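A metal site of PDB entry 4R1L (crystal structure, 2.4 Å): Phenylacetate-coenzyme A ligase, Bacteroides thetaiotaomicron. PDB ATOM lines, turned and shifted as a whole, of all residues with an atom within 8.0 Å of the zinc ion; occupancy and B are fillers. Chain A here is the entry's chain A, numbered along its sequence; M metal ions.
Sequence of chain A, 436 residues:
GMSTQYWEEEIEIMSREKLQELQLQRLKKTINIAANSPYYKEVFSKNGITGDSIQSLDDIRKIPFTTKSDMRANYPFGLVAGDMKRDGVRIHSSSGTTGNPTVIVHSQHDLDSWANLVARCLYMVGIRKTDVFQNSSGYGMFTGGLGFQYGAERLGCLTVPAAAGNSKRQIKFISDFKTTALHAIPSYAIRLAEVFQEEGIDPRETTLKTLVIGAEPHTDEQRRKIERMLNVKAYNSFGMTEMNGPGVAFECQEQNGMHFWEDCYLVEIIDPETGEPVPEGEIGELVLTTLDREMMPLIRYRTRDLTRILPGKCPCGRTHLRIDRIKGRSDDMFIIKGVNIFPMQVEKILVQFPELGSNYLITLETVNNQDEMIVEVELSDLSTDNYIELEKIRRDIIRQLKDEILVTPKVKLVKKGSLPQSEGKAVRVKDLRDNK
ND1 of His 259 sits at hydrogen-bond distance from O of His 320 (2.8 Å). O of Phe 250 is in hydrogen-bond range of N of His 259 (2.8 Å). The guanidinium group (NH1) of Arg 318 sits close to the side-chain sulfur (SG) of Cys 316. O of Cys 316 sits at hydrogen-bond distance from OH of Tyr 6 (2.7 Å). SG of Cys 252 sits close to N of Glu 254, at 3.5 Å.
Within 4 Å of the zinc ion: Cys 252, His 259, Cys 314 and Cys 316. The nearest printed residue that does not touch the zinc ion is Glu 254 (4.5 Å).
The zinc ion is bound by a ring nitrogen (NE2) of His 259 (2.1 Å), the side-chain sulfur of Cys 316 (2.2 Å), the side-chain sulfur of Cys 252 (2.3 Å) and the side-chain sulfur of Cys 314 (2.5 Å). The zinc ion has four donor atoms within binding distance.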
ATOM      1  N   THR A   4     -21.276   4.734  36.626  1.00  0.00           N
ATOM      2  CA  THR A   4     -22.342   4.386  35.677  1.00  0.00           C
ATOM      3  C   THR A   4     -23.600   3.900  36.449  1.00  0.00           C
ATOM      4  O   THR A   4     -23.483   3.141  37.416  1.00  0.00           O
ATOM      5  CB  THR A   4     -21.880   3.313  34.648  1.00  0.00           C
ATOM      6  OG1 THR A   4     -20.715   3.797  33.996  1.00  0.00           O
ATOM      7  CG2 THR A   4     -22.904   3.029  33.575  1.00  0.00           C
ATOM      8  N   TYR A   6     -27.608   2.233  36.088  1.00  0.00           N
ATOM      9  CA  TYR A   6     -28.415   1.335  35.277  1.00  0.00           C
ATOM     10  C   TYR A   6     -29.890   1.323  35.732  1.00  0.00           C
ATOM     11  O   TYR A   6     -30.182   1.396  36.919  1.00  0.00           O
ATOM     12  CB  TYR A   6     -27.840  -0.093  35.361  1.00  0.00           C
ATOM     13  CG  TYR A   6     -26.337  -0.165  35.181  1.00  0.00           C
ATOM     14  CD1 TYR A   6     -25.767  -0.213  33.904  1.00  0.00           C
ATOM     15  CD2 TYR A   6     -25.477  -0.179  36.276  1.00  0.00           C
ATOM     16  CE1 TYR A   6     -24.385  -0.263  33.733  1.00  0.00           C
ATOM     17  CE2 TYR A   6     -24.093  -0.237  36.116  1.00  0.00           C
ATOM     18  CZ  TYR A   6     -23.555  -0.275  34.836  1.00  0.00           C
ATOM     19  OH  TYR A   6     -22.202  -0.303  34.670  1.00  0.00           O
ATOM     20  N   MET A 124     -30.334   4.929  30.414  1.00  0.00           N
ATOM     21  CA  MET A 124     -28.944   4.660  30.040  1.00  0.00           C
ATOM     22  C   MET A 124     -28.219   5.916  29.541  1.00  0.00           C
ATOM     23  O   MET A 124     -27.034   6.109  29.873  1.00  0.00           O
ATOM     24  CB  MET A 124     -28.890   3.584  28.956  1.00  0.00           C
ATOM     25  CG  MET A 124     -27.472   3.293  28.420  1.00  0.00           C
ATOM     26  SD  MET A 124     -27.366   1.670  27.394  1.00  0.00           S
ATOM     27  CE  MET A 124     -28.531   2.117  25.970  1.00  0.00           C
ATOM     28  N   PHE A 250     -29.570   0.769  21.364  1.00  0.00           N
ATOM     29  CA  PHE A 250     -29.349   2.157  21.716  1.00  0.00           C
ATOM     30  C   PHE A 250     -27.926   2.401  22.153  1.00  0.00           C
ATOM     31  O   PHE A 250     -27.352   1.547  22.830  1.00  0.00           O
ATOM     32  CB  PHE A 250     -30.319   2.476  22.878  1.00  0.00           C
ATOM     33  CG  PHE A 250     -31.065   3.792  22.917  1.00  0.00           C
ATOM     34  CD1 PHE A 250     -32.325   3.909  22.325  1.00  0.00           C
ATOM     35  CD2 PHE A 250     -30.593   4.859  23.682  1.00  0.00           C
ATOM     36  CE1 PHE A 250     -33.080   5.078  22.470  1.00  0.00           C
ATOM     37  CE2 PHE A 250     -31.331   6.036  23.811  1.00  0.00           C
ATOM     38  CZ  PHE A 250     -32.582   6.132  23.219  1.00  0.00           C
ATOM     39  N   GLU A 251     -27.372   3.579  21.805  1.00  0.00           N
ATOM     40  CA  GLU A 251     -26.030   3.949  22.269  1.00  0.00           C
ATOM     41  C   GLU A 251     -26.006   4.180  23.757  1.00  0.00           C
ATOM     42  O   GLU A 251     -27.015   4.572  24.335  1.00  0.00           O
ATOM     43  CB  GLU A 251     -25.512   5.221  21.573  1.00  0.00           C
ATOM     44  CG  GLU A 251     -24.945   5.047  20.189  1.00  0.00           C
ATOM     45  CD  GLU A 251     -24.450   6.384  19.668  1.00  0.00           C
ATOM     46  OE1 GLU A 251     -25.158   7.388  19.864  1.00  0.00           O
ATOM     47  OE2 GLU A 251     -23.351   6.433  19.081  1.00  0.00           O
ATOM     48  N   CYS A 252     -24.854   3.979  24.389  1.00  0.00           N
ATOM     49  CA  CYS A 252     -24.680   4.310  25.803  1.00  0.00           C
ATOM     50  C   CYS A 252     -24.031   5.701  25.850  1.00  0.00           C
ATOM     51  O   CYS A 252     -23.907   6.335  24.803  1.00  0.00           O
ATOM     52  CB  CYS A 252     -23.862   3.249  26.536  1.00  0.00           C
ATOM     53  SG  CYS A 252     -22.173   3.054  25.914  1.00  0.00           S
ATOM     54  N   GLN A 253     -23.576   6.176  27.011  1.00  0.00           N
ATOM     55  CA  GLN A 253     -22.984   7.506  27.051  1.00  0.00           C
ATOM     56  C   GLN A 253     -21.581   7.504  26.408  1.00  0.00           C
ATOM     57  O   GLN A 253     -21.053   8.586  26.174  1.00  0.00           O
ATOM     58  CB  GLN A 253     -22.943   8.061  28.471  1.00  0.00           C
ATOM     59  CG  GLN A 253     -24.367   8.344  28.946  1.00  0.00           C
ATOM     60  CD  GLN A 253     -24.484   8.933  30.311  1.00  0.00           C
ATOM     61  OE1 GLN A 253     -25.384   8.574  31.083  1.00  0.00           O
ATOM     62  NE2 GLN A 253     -23.628   9.895  30.630  1.00  0.00           N
ATOM     63  N   GLU A 254     -21.031   6.317  26.039  1.00  0.00           N
ATOM     64  CA  GLU A 254     -19.754   6.187  25.333  1.00  0.00           C
ATOM     65  C   GLU A 254     -19.891   6.618  23.882  1.00  0.00           C
ATOM     66  O   GLU A 254     -18.893   6.935  23.255  1.00  0.00           O
ATOM     67  CB  GLU A 254     -19.205   4.746  25.395  1.00  0.00           C
ATOM     68  CG  GLU A 254     -18.786   4.292  26.782  1.00  0.00           C
ATOM     69  CD  GLU A 254     -17.668   5.082  27.419  1.00  0.00           C
ATOM     70  OE1 GLU A 254     -16.623   5.302  26.750  1.00  0.00           O
ATOM     71  OE2 GLU A 254     -17.812   5.465  28.598  1.00  0.00           O
ATOM     72  N   GLN A 255     -21.145   6.599  23.338  1.00  0.00           N
ATOM     73  CA  GLN A 255     -21.473   6.962  21.958  1.00  0.00           C
ATOM     74  C   GLN A 255     -20.588   6.184  20.985  1.00  0.00           C
ATOM     75  O   GLN A 255     -19.969   6.772  20.091  1.00  0.00           O
ATOM     76  CB  GLN A 255     -21.349   8.482  21.724  1.00  0.00           C
ATOM     77  CG  GLN A 255     -22.353   9.308  22.515  1.00  0.00           C
ATOM     78  CD  GLN A 255     -22.207  10.779  22.218  1.00  0.00           C
ATOM     79  OE1 GLN A 255     -21.104  11.356  22.249  1.00  0.00           O
ATOM     80  NE2 GLN A 255     -23.330  11.435  21.967  1.00  0.00           N
ATOM     81  N   ASN A 256     -20.499   4.861  21.208  1.00  0.00           N
ATOM     82  CA  ASN A 256     -19.690   3.964  20.396  1.00  0.00           C
ATOM     83  C   ASN A 256     -20.341   2.581  20.338  1.00  0.00           C
ATOM     84  O   ASN A 256     -20.001   1.684  21.116  1.00  0.00           O
ATOM     85  CB  ASN A 256     -18.251   3.896  20.912  1.00  0.00           C
ATOM     86  CG  ASN A 256     -17.337   3.005  20.071  1.00  0.00           C
ATOM     87  OD1 ASN A 256     -16.476   2.323  20.626  1.00  0.00           O
ATOM     88  ND2 ASN A 256     -17.576   2.921  18.757  1.00  0.00           N
ATOM     89  N   GLY A 257     -21.254   2.453  19.381  1.00  0.00           N
ATOM     90  CA  GLY A 257     -22.015   1.240  19.152  1.00  0.00           C
ATOM     91  C   GLY A 257     -23.314   1.267  19.910  1.00  0.00           C
ATOM     92  O   GLY A 257     -23.429   1.905  20.964  1.00  0.00           O
ATOM     93  N   MET A 258     -24.320   0.609  19.361  1.00  0.00           N
ATOM     94  CA  MET A 258     -25.643   0.535  19.971  1.00  0.00           C
ATOM     95  C   MET A 258     -25.821  -0.796  20.707  1.00  0.00           C
ATOM     96  O   MET A 258     -25.813  -1.871  20.074  1.00  0.00           O
ATOM     97  CB  MET A 258     -26.733   0.708  18.918  1.00  0.00           C
ATOM     98  CG  MET A 258     -26.814   2.142  18.395  1.00  0.00           C
ATOM     99  SD  MET A 258     -28.186   2.345  17.091  1.00  0.00           S
ATOM    100  CE  MET A 258     -27.386   1.491  15.618  1.00  0.00           C
ATOM    101  N   HIS A 259     -25.977  -0.723  22.056  1.00  0.00           N
ATOM    102  CA  HIS A 259     -26.253  -1.887  22.902  1.00  0.00           C
ATOM    103  C   HIS A 259     -27.598  -2.519  22.515  1.00  0.00           C
ATOM    104  O   HIS A 259     -28.618  -1.834  22.493  1.00  0.00           O
ATOM    105  CB  HIS A 259     -26.255  -1.514  24.388  1.00  0.00           C
ATOM    106  CG  HIS A 259     -24.881  -1.292  24.957  1.00  0.00           C
ATOM    107  ND1 HIS A 259     -24.052  -2.360  25.269  1.00  0.00           N
ATOM    108  CD2 HIS A 259     -24.246  -0.137  25.269  1.00  0.00           C
ATOM    109  CE1 HIS A 259     -22.935  -1.823  25.751  1.00  0.00           C
ATOM    110  NE2 HIS A 259     -23.010  -0.497  25.775  1.00  0.00           N
ATOM    111  N   TRP A 261     -30.522  -5.209  23.415  1.00  0.00           N
ATOM    112  CA  TRP A 261     -30.966  -5.842  24.664  1.00  0.00           C
ATOM    113  C   TRP A 261     -31.216  -7.316  24.415  1.00  0.00           C
ATOM    114  O   TRP A 261     -32.299  -7.733  24.001  1.00  0.00           O
ATOM    115  CB  TRP A 261     -32.185  -5.138  25.289  1.00  0.00           C
ATOM    116  CG  TRP A 261     -31.890  -3.692  25.634  1.00  0.00           C
ATOM    117  CD1 TRP A 261     -32.457  -2.603  25.060  1.00  0.00           C
ATOM    118  CD2 TRP A 261     -30.812  -3.211  26.448  1.00  0.00           C
ATOM    119  NE1 TRP A 261     -31.877  -1.453  25.554  1.00  0.00           N
ATOM    120  CE2 TRP A 261     -30.844  -1.796  26.384  1.00  0.00           C
ATOM    121  CE3 TRP A 261     -29.837  -3.828  27.267  1.00  0.00           C
ATOM    122  CZ2 TRP A 261     -29.964  -0.989  27.135  1.00  0.00           C
ATOM    123  CZ3 TRP A 261     -28.952  -3.034  27.997  1.00  0.00           C
ATOM    124  CH2 TRP A 261     -29.021  -1.631  27.914  1.00  0.00           C
ATOM    125  N   LYS A 313     -15.122  -5.283  25.096  1.00  0.00           N
ATOM    126  CA  LYS A 313     -15.956  -4.870  26.209  1.00  0.00           C
ATOM    127  C   LYS A 313     -16.252  -3.366  26.112  1.00  0.00           C
ATOM    128  O   LYS A 313     -15.411  -2.628  25.598  1.00  0.00           O
ATOM    129  CB  LYS A 313     -15.281  -5.190  27.562  1.00  0.00           C
ATOM    130  CG  LYS A 313     -15.044  -6.666  27.859  1.00  0.00           C
ATOM    131  CD  LYS A 313     -14.427  -6.870  29.243  1.00  0.00           C
ATOM    132  CE  LYS A 313     -14.303  -8.324  29.621  1.00  0.00           C
ATOM    133  NZ  LYS A 313     -13.751  -8.469  30.984  1.00  0.00           N
ATOM    134  N   CYS A 314     -17.407  -2.918  26.638  1.00  0.00           N
ATOM    135  CA  CYS A 314     -17.673  -1.484  26.626  1.00  0.00           C
ATOM    136  C   CYS A 314     -17.302  -0.880  27.992  1.00  0.00           C
ATOM    137  O   CYS A 314     -17.669  -1.464  29.015  1.00  0.00           O
ATOM    138  CB  CYS A 314     -19.123  -1.164  26.257  1.00  0.00           C
ATOM    139  SG  CYS A 314     -19.438   0.622  26.076  1.00  0.00           S
ATOM    140  N   PRO A 315     -16.654   0.309  28.034  1.00  0.00           N
ATOM    141  CA  PRO A 315     -16.332   0.944  29.326  1.00  0.00           C
ATOM    142  C   PRO A 315     -17.565   1.269  30.203  1.00  0.00           C
ATOM    143  O   PRO A 315     -17.352   1.547  31.383  1.00  0.00           O
ATOM    144  CB  PRO A 315     -15.644   2.253  28.913  1.00  0.00           C
ATOM    145  CG  PRO A 315     -15.112   2.014  27.567  1.00  0.00           C
ATOM    146  CD  PRO A 315     -16.128   1.119  26.907  1.00  0.00           C
ATOM    147  N   CYS A 316     -18.831   1.220  29.656  1.00  0.00           N
ATOM    148  CA  CYS A 316     -20.017   1.507  30.483  1.00  0.00           C
ATOM    149  C   CYS A 316     -20.302   0.315  31.418  1.00  0.00           C
ATOM    150  O   CYS A 316     -21.067   0.453  32.371  1.00  0.00           O
ATOM    151  CB  CYS A 316     -21.246   1.883  29.650  1.00  0.00           C
ATOM    152  SG  CYS A 316     -22.063   0.488  28.813  1.00  0.00           S
ATOM    153  N   GLY A 317     -19.660  -0.828  31.154  1.00  0.00           N
ATOM    154  CA  GLY A 317     -19.797  -2.041  31.947  1.00  0.00           C
ATOM    155  C   GLY A 317     -20.930  -2.945  31.508  1.00  0.00           C
ATOM    156  O   GLY A 317     -21.082  -4.038  32.069  1.00  0.00           O
ATOM    157  N   ARG A 318     -21.739  -2.523  30.533  1.00  0.00           N
ATOM    158  CA  ARG A 318     -22.831  -3.353  30.041  1.00  0.00           C
ATOM    159  C   ARG A 318     -22.255  -4.486  29.178  1.00  0.00           C
ATOM    160  O   ARG A 318     -21.284  -4.286  28.427  1.00  0.00           O
ATOM    161  CB  ARG A 318     -23.895  -2.545  29.284  1.00  0.00           C
ATOM    162  CG  ARG A 318     -24.654  -1.611  30.234  1.00  0.00           C
ATOM    163  CD  ARG A 318     -25.603  -0.709  29.506  1.00  0.00           C
ATOM    164  NE  ARG A 318     -26.325   0.188  30.409  1.00  0.00           N
ATOM    165  CZ  ARG A 318     -25.887   1.385  30.790  1.00  0.00           C
ATOM    166  NH1 ARG A 318     -24.716   1.838  30.360  1.00  0.00           N
ATOM    167  NH2 ARG A 318     -26.607   2.130  31.609  1.00  0.00           N
ATOM    168  N   THR A 319     -22.797  -5.684  29.379  1.00  0.00           N
ATOM    169  CA  THR A 319     -22.369  -6.933  28.758  1.00  0.00           C
ATOM    170  C   THR A 319     -23.137  -7.248  27.484  1.00  0.00           C
ATOM    171  O   THR A 319     -22.769  -8.176  26.775  1.00  0.00           O
ATOM    172  CB  THR A 319     -22.559  -8.067  29.764  1.00  0.00           C
ATOM    173  OG1 THR A 319     -23.899  -8.000  30.287  1.00  0.00           O
ATOM    174  CG2 THR A 319     -21.532  -8.002  30.929  1.00  0.00           C
ATOM    175  N   HIS A 320     -24.220  -6.495  27.209  1.00  0.00           N
ATOM    176  CA  HIS A 320     -25.036  -6.679  26.003  1.00  0.00           C
ATOM    177  C   HIS A 320     -24.262  -6.208  24.779  1.00  0.00           C
ATOM    178  O   HIS A 320     -23.717  -5.092  24.797  1.00  0.00           O
ATOM    179  CB  HIS A 320     -26.369  -5.917  26.150  1.00  0.00           C
ATOM    180  CG  HIS A 320     -27.248  -6.512  27.199  1.00  0.00           C
ATOM    181  ND1 HIS A 320     -28.349  -7.282  26.858  1.00  0.00           N
ATOM    182  CD2 HIS A 320     -27.119  -6.503  28.542  1.00  0.00           C
ATOM    183  CE1 HIS A 320     -28.881  -7.675  28.006  1.00  0.00           C
ATOM    184  NE2 HIS A 320     -28.159  -7.240  29.047  1.00  0.00           N
ATOM    185  N   ARG A 322     -22.934  -4.768  21.136  1.00  0.00           N
ATOM    186  CA  ARG A 322     -23.071  -3.500  20.431  1.00  0.00           C
ATOM    187  C   ARG A 322     -23.009  -3.721  18.950  1.00  0.00           C
ATOM    188  O   ARG A 322     -22.140  -4.454  18.455  1.00  0.00           O
ATOM    189  CB  ARG A 322     -21.981  -2.497  20.848  1.00  0.00           C
ATOM    190  CG  ARG A 322     -22.093  -1.989  22.285  1.00  0.00           C
ATOM    191  CD  ARG A 322     -20.836  -1.313  22.762  1.00  0.00           C
ATOM    192  NE  ARG A 322     -19.691  -2.217  22.748  1.00  0.00           N
ATOM    193  CZ  ARG A 322     -18.650  -2.088  21.926  1.00  0.00           C
ATOM    194  NH1 ARG A 322     -18.555  -1.047  21.125  1.00  0.00           N
ATOM    195  NH2 ARG A 322     -17.670  -2.973  21.953  1.00  0.00           N
HETATM  196 ZN    ZN M   1     -21.830   0.944  26.684  1.00  0.00          ZN
